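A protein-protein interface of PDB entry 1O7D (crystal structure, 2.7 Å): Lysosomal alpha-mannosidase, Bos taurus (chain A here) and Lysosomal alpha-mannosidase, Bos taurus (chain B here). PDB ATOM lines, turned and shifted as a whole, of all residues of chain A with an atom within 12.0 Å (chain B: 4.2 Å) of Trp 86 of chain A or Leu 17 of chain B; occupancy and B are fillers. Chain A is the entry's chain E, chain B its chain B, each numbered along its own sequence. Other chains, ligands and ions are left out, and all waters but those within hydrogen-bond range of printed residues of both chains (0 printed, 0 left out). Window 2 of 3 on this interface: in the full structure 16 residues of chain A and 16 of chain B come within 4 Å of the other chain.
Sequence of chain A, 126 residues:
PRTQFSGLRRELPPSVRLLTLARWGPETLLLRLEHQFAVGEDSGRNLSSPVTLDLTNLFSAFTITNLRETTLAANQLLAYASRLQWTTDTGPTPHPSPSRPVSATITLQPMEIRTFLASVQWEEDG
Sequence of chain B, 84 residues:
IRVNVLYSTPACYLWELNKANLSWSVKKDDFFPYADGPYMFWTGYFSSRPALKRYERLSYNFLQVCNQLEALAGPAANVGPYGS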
ATOM      1  N   SER A  82      13.852  -3.235 -20.225  1.00  0.00           N
ATOM      2  CA  SER A  82      14.126  -2.574 -21.490  1.00  0.00           C
ATOM      3  C   SER A  82      13.091  -1.486 -21.733  1.00  0.00           C
ATOM      4  O   SER A  82      11.978  -1.549 -21.216  1.00  0.00           O
ATOM      5  CB  SER A  82      14.094  -3.589 -22.649  1.00  0.00           C
ATOM      6  OG  SER A  82      12.840  -4.258 -22.739  1.00  0.00           O
ATOM      7  N   ARG A  83      13.466  -0.495 -22.526  1.00  0.00           N
ATOM      8  CA  ARG A  83      12.584   0.615 -22.856  1.00  0.00           C
ATOM      9  C   ARG A  83      12.471   0.762 -24.370  1.00  0.00           C
ATOM     10  O   ARG A  83      13.368   0.352 -25.089  1.00  0.00           O
ATOM     11  CB  ARG A  83      13.156   1.897 -22.263  1.00  0.00           C
ATOM     12  CG  ARG A  83      12.896   2.068 -20.777  1.00  0.00           C
ATOM     13  CD  ARG A  83      14.096   2.713 -20.088  1.00  0.00           C
ATOM     14  NE  ARG A  83      14.698   3.798 -20.868  1.00  0.00           N
ATOM     15  CZ  ARG A  83      14.182   5.018 -20.997  1.00  0.00           C
ATOM     16  NH1 ARG A  83      13.045   5.345 -20.403  1.00  0.00           N
ATOM     17  NH2 ARG A  83      14.810   5.922 -21.729  1.00  0.00           N
ATOM     18  N   LEU A  84      11.381   1.346 -24.855  1.00  0.00           N
ATOM     19  CA  LEU A  84      11.202   1.528 -26.291  1.00  0.00           C
ATOM     20  C   LEU A  84      12.289   2.473 -26.800  1.00  0.00           C
ATOM     21  O   LEU A  84      12.739   3.351 -26.064  1.00  0.00           O
ATOM     22  CB  LEU A  84       9.837   2.148 -26.574  1.00  0.00           C
ATOM     23  CG  LEU A  84       8.601   1.576 -25.881  1.00  0.00           C
ATOM     24  CD1 LEU A  84       7.368   2.352 -26.349  1.00  0.00           C
ATOM     25  CD2 LEU A  84       8.453   0.108 -26.202  1.00  0.00           C
ATOM     26  N   GLN A  85      12.722   2.310 -28.044  1.00  0.00           N
ATOM     27  CA  GLN A  85      13.747   3.210 -28.569  1.00  0.00           C
ATOM     28  C   GLN A  85      13.122   4.384 -29.324  1.00  0.00           C
ATOM     29  O   GLN A  85      11.971   4.303 -29.742  1.00  0.00           O
ATOM     30  CB  GLN A  85      14.715   2.433 -29.454  1.00  0.00           C
ATOM     31  CG  GLN A  85      15.459   1.349 -28.699  1.00  0.00           C
ATOM     32  CD  GLN A  85      16.445   1.901 -27.719  1.00  0.00           C
ATOM     33  OE1 GLN A  85      17.620   2.322 -28.090  1.00  0.00           O
ATOM     34  NE2 GLN A  85      16.041   1.929 -26.428  1.00  0.00           N
ATOM     35  N   TRP A  86      13.869   5.476 -29.473  1.00  0.00           N
ATOM     36  CA  TRP A  86      13.358   6.661 -30.158  1.00  0.00           C
ATOM     37  C   TRP A  86      14.403   7.370 -31.021  1.00  0.00           C
ATOM     38  O   TRP A  86      15.479   7.750 -30.542  1.00  0.00           O
ATOM     39  CB  TRP A  86      12.792   7.657 -29.137  1.00  0.00           C
ATOM     40  CG  TRP A  86      11.655   7.121 -28.366  1.00  0.00           C
ATOM     41  CD1 TRP A  86      11.706   6.527 -27.151  1.00  0.00           C
ATOM     42  CD2 TRP A  86      10.296   7.052 -28.794  1.00  0.00           C
ATOM     43  NE1 TRP A  86      10.462   6.084 -26.787  1.00  0.00           N
ATOM     44  CE2 TRP A  86       9.577   6.393 -27.783  1.00  0.00           C
ATOM     45  CE3 TRP A  86       9.617   7.484 -29.936  1.00  0.00           C
ATOM     46  CZ2 TRP A  86       8.206   6.147 -27.881  1.00  0.00           C
ATOM     47  CZ3 TRP A  86       8.262   7.241 -30.034  1.00  0.00           C
ATOM     48  CH2 TRP A  86       7.569   6.578 -29.013  1.00  0.00           C
ATOM     49  N   THR A  87      14.083   7.568 -32.292  1.00  0.00           N
ATOM     50  CA  THR A  87      15.015   8.231 -33.200  1.00  0.00           C
ATOM     51  C   THR A  87      14.887   9.735 -33.116  1.00  0.00           C
ATOM     52  O   THR A  87      13.825  10.280 -33.404  1.00  0.00           O
ATOM     53  CB  THR A  87      14.756   7.851 -34.677  1.00  0.00           C
ATOM     54  OG1 THR A  87      14.889   6.440 -34.844  1.00  0.00           O
ATOM     55  CG2 THR A  87      15.744   8.558 -35.595  1.00  0.00           C
ATOM     56  N   THR A  88      15.967  10.405 -32.737  1.00  0.00           N
ATOM     57  CA  THR A  88      15.950  11.857 -32.676  1.00  0.00           C
ATOM     58  C   THR A  88      16.747  12.362 -33.875  1.00  0.00           C
ATOM     59  O   THR A  88      17.776  11.782 -34.207  1.00  0.00           O
ATOM     60  CB  THR A  88      16.591  12.361 -31.379  1.00  0.00           C
ATOM     61  OG1 THR A  88      17.967  11.954 -31.330  1.00  0.00           O
ATOM     62  CG2 THR A  88      15.841  11.792 -30.171  1.00  0.00           C
ATOM     63  N   ASP A  89      16.262  13.415 -34.534  1.00  0.00           N
ATOM     64  CA  ASP A  89      16.943  13.983 -35.704  1.00  0.00           C
ATOM     65  C   ASP A  89      17.726  15.234 -35.354  1.00  0.00           C
ATOM     66  O   ASP A  89      17.901  15.540 -34.182  1.00  0.00           O
ATOM     67  CB  ASP A  89      15.940  14.314 -36.816  1.00  0.00           C
ATOM     68  CG  ASP A  89      14.755  15.132 -36.321  1.00  0.00           C
ATOM     69  OD1 ASP A  89      14.960  16.254 -35.791  1.00  0.00           O
ATOM     70  OD2 ASP A  89      13.607  14.647 -36.468  1.00  0.00           O
ATOM     71  N   TYR B  13      -1.338   4.300 -26.801  1.00  0.00           N
ATOM     72  CA  TYR B  13      -1.207   5.423 -27.710  1.00  0.00           C
ATOM     73  C   TYR B  13       0.283   5.647 -27.963  1.00  0.00           C
ATOM     74  O   TYR B  13       0.695   6.113 -29.030  1.00  0.00           O
ATOM     75  CB  TYR B  13      -1.836   6.677 -27.088  1.00  0.00           C
ATOM     76  CG  TYR B  13      -1.418   7.957 -27.756  1.00  0.00           C
ATOM     77  CD1 TYR B  13      -1.720   8.191 -29.098  1.00  0.00           C
ATOM     78  CD2 TYR B  13      -0.692   8.921 -27.063  1.00  0.00           C
ATOM     79  CE1 TYR B  13      -1.306   9.362 -29.746  1.00  0.00           C
ATOM     80  CE2 TYR B  13      -0.266  10.093 -27.694  1.00  0.00           C
ATOM     81  CZ  TYR B  13      -0.582  10.310 -29.041  1.00  0.00           C
ATOM     82  OH  TYR B  13      -0.199  11.479 -29.683  1.00  0.00           O
ATOM     83  N   LEU B  14       1.096   5.299 -26.977  1.00  0.00           N
ATOM     84  CA  LEU B  14       2.525   5.492 -27.119  1.00  0.00           C
ATOM     85  C   LEU B  14       3.108   4.395 -27.977  1.00  0.00           C
ATOM     86  O   LEU B  14       4.073   4.628 -28.716  1.00  0.00           O
ATOM     87  CB  LEU B  14       3.226   5.504 -25.755  1.00  0.00           C
ATOM     88  CG  LEU B  14       4.633   6.120 -25.807  1.00  0.00           C
ATOM     89  CD1 LEU B  14       4.525   7.624 -26.028  1.00  0.00           C
ATOM     90  CD2 LEU B  14       5.370   5.851 -24.532  1.00  0.00           C
ATOM     91  N   TRP B  15       2.533   3.197 -27.886  1.00  0.00           N
ATOM     92  CA  TRP B  15       3.035   2.099 -28.690  1.00  0.00           C
ATOM     93  C   TRP B  15       2.832   2.427 -30.156  1.00  0.00           C
ATOM     94  O   TRP B  15       3.692   2.141 -30.980  1.00  0.00           O
ATOM     95  CB  TRP B  15       2.322   0.795 -28.336  1.00  0.00           C
ATOM     96  CG  TRP B  15       2.801  -0.393 -29.125  1.00  0.00           C
ATOM     97  CD1 TRP B  15       2.017  -1.329 -29.723  1.00  0.00           C
ATOM     98  CD2 TRP B  15       4.165  -0.759 -29.428  1.00  0.00           C
ATOM     99  NE1 TRP B  15       2.795  -2.254 -30.383  1.00  0.00           N
ATOM    100  CE2 TRP B  15       4.120  -1.930 -30.217  1.00  0.00           C
ATOM    101  CE3 TRP B  15       5.420  -0.210 -29.112  1.00  0.00           C
ATOM    102  CZ2 TRP B  15       5.277  -2.566 -30.706  1.00  0.00           C
ATOM    103  CZ3 TRP B  15       6.580  -0.841 -29.601  1.00  0.00           C
ATOM    104  CH2 TRP B  15       6.495  -2.008 -30.387  1.00  0.00           C
ATOM    105  N   GLU B  16       1.718   3.070 -30.483  1.00  0.00           N
ATOM    106  CA  GLU B  16       1.471   3.406 -31.884  1.00  0.00           C
ATOM    107  C   GLU B  16       2.455   4.459 -32.353  1.00  0.00           C
ATOM    108  O   GLU B  16       2.917   4.419 -33.486  1.00  0.00           O
ATOM    109  CB  GLU B  16       0.032   3.908 -32.060  1.00  0.00           C
ATOM    110  CG  GLU B  16      -1.025   2.845 -31.935  1.00  0.00           C
ATOM    111  CD  GLU B  16      -0.747   1.627 -32.808  1.00  0.00           C
ATOM    112  OE1 GLU B  16      -0.403   1.780 -34.008  1.00  0.00           O
ATOM    113  OE2 GLU B  16      -0.891   0.502 -32.287  1.00  0.00           O
ATOM    114  N   LEU B  17       2.789   5.401 -31.478  1.00  0.00           N
ATOM    115  CA  LEU B  17       3.720   6.465 -31.860  1.00  0.00           C
ATOM    116  C   LEU B  17       5.089   5.881 -32.139  1.00  0.00           C
ATOM    117  O   LEU B  17       5.823   6.348 -33.007  1.00  0.00           O
ATOM    118  CB  LEU B  17       3.816   7.526 -30.753  1.00  0.00           C
ATOM    119  CG  LEU B  17       2.483   8.149 -30.310  1.00  0.00           C
ATOM    120  CD1 LEU B  17       2.762   9.243 -29.261  1.00  0.00           C
ATOM    121  CD2 LEU B  17       1.739   8.723 -31.515  1.00  0.00           C
ATOM    122  N   ASN B  18       5.437   4.841 -31.397  1.00  0.00           N
ATOM    123  CA  ASN B  18       6.724   4.206 -31.611  1.00  0.00           C
ATOM    124  C   ASN B  18       6.687   3.483 -32.961  1.00  0.00           C
ATOM    125  O   ASN B  18       7.547   3.698 -33.809  1.00  0.00           O
ATOM    126  CB  ASN B  18       7.013   3.228 -30.465  1.00  0.00           C
ATOM    127  CG  ASN B  18       8.463   2.788 -30.423  1.00  0.00           C
ATOM    128  OD1 ASN B  18       8.796   1.690 -30.853  1.00  0.00           O
ATOM    129  ND2 ASN B  18       9.331   3.648 -29.911  1.00  0.00           N
ATOM    130  N   LYS B  19       5.660   2.655 -33.154  1.00  0.00           N
ATOM    131  CA  LYS B  19       5.470   1.865 -34.378  1.00  0.00           C
ATOM    132  C   LYS B  19       5.630   2.667 -35.650  1.00  0.00           C
ATOM    133  O   LYS B  19       5.962   2.114 -36.693  1.00  0.00           O
ATOM    134  CB  LYS B  19       4.079   1.220 -34.412  1.00  0.00           C
ATOM    135  CG  LYS B  19       3.762   0.334 -33.222  1.00  0.00           C
ATOM    136  CD  LYS B  19       2.337  -0.206 -33.292  1.00  0.00           C
ATOM    137  CE  LYS B  19       2.253  -1.389 -34.245  1.00  0.00           C
ATOM    138  NZ  LYS B  19       3.080  -2.545 -33.713  1.00  0.00           N
ATOM    139  N   ALA B  20       5.395   3.968 -35.572  1.00  0.00           N
ATOM    140  CA  ALA B  20       5.506   4.802 -36.747  1.00  0.00           C
ATOM    141  C   ALA B  20       6.921   5.059 -37.221  1.00  0.00           C
ATOM    142  O   ALA B  20       7.105   5.529 -38.329  1.00  0.00           O
ATOM    143  CB  ALA B  20       4.815   6.112 -36.499  1.00  0.00           C
ATOM    144  N   TRP B  24      11.990  12.478 -33.983  1.00  0.00           N
ATOM    145  CA  TRP B  24      11.507  13.607 -33.220  1.00  0.00           C
ATOM    146  C   TRP B  24      12.586  14.603 -32.835  1.00  0.00           C
ATOM    147  O   TRP B  24      13.761  14.251 -32.722  1.00  0.00           O
ATOM    148  CB  TRP B  24      10.791  13.094 -31.978  1.00  0.00           C
ATOM    149  CG  TRP B  24       9.417  12.549 -32.282  1.00  0.00           C
ATOM    150  CD1 TRP B  24       8.218  13.246 -32.297  1.00  0.00           C
ATOM    151  CD2 TRP B  24       9.091  11.194 -32.581  1.00  0.00           C
ATOM    152  NE1 TRP B  24       7.172  12.393 -32.576  1.00  0.00           N
ATOM    153  CE2 TRP B  24       7.676  11.128 -32.755  1.00  0.00           C
ATOM    154  CE3 TRP B  24       9.851  10.022 -32.714  1.00  0.00           C
ATOM    155  CZ2 TRP B  24       7.017   9.934 -33.050  1.00  0.00           C
ATOM    156  CZ3 TRP B  24       9.196   8.834 -33.008  1.00  0.00           C
ATOM    157  CH2 TRP B  24       7.792   8.798 -33.173  1.00  0.00           C
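O of Trp 24 of chain B lies within hydrogen-bond range of N of Asp 89 of chain A (3.2 Å). N of Trp 24 of chain B sits at hydrogen-bond distance from O of Thr 87 of chain A, 2.9 Å away. O of Gln 85 of chain A is in hydrogen-bond range of ND2 of Asn 18 of chain B (2.7 Å).
The side-chain amide nitrogen of Gln 85 of chain A is in hydrogen-bond range of the backbone carbonyl oxygen of Arg 83 of chain A (3.4 Å).
Among the printed residues, merely in contact across the chains: Thr 88 of chain A with Trp 24 of chain B (3.2 Å), Trp 86 of chain A with Trp 24 of chain B (3.4 Å), Trp 86 of chain A with Asn 18 of chain B (3.4 Å), Leu 84 of chain A with Asn 18 of chain B (3.7 Å), Trp 86 of chain A with Leu 17 of chain B (3.9 Å) and Leu 84 of chain A with Trp 15 of chain B (3.995 Å).
Ser 82 of chain A touches none of the printed residues of chain B. Printed residues of chain B within 4 Å of Gln 85 of chain A: Asn 18. Of the printed residues of chain B, Thr 87 of chain A touches Trp 24 (2.9 Å). Of the printed residues of chain B, Thr 88 of chain A touches Trp 24. Of the printed residues of chain B, Asp 89 of chain A touches Trp 24. No residue of chain A comes within 4 Å of Tyr 13 of chain B. Of the printed residues of chain A, Trp 15 of chain B touches Leu 84 (3.995 Å). Of chain A, only Trp 86 comes within 4 Å of Leu 17 of chain B. Asn 18 of chain B touches three residues of chain A. No residue of chain A comes within 4 Å of Ala 20 of chain B. Of chain A, only Trp 86, Thr 87, Thr 88 and Asp 89 come within 4 Å of Trp 24 of chain B. The nearest printed residue of chain B that does not touch Trp 86 of chain A is Leu 14 of chain B (4.01 Å).
Printed residues of chain B that touch a printed residue of chain A: Trp 15, Leu 17, Asn 18 and Trp 24. Hydrophobic or aromatic side chains of chain B within 4 Å of the printed part of chain A: Trp 15 and Trp 24. Printed residues of chain A that touch a printed residue of chain B: Leu 84, Gln 85, Trp 86, Thr 87, Thr 88 and Asp 89. Among the printed residues, 9 pairs touch across the chains.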
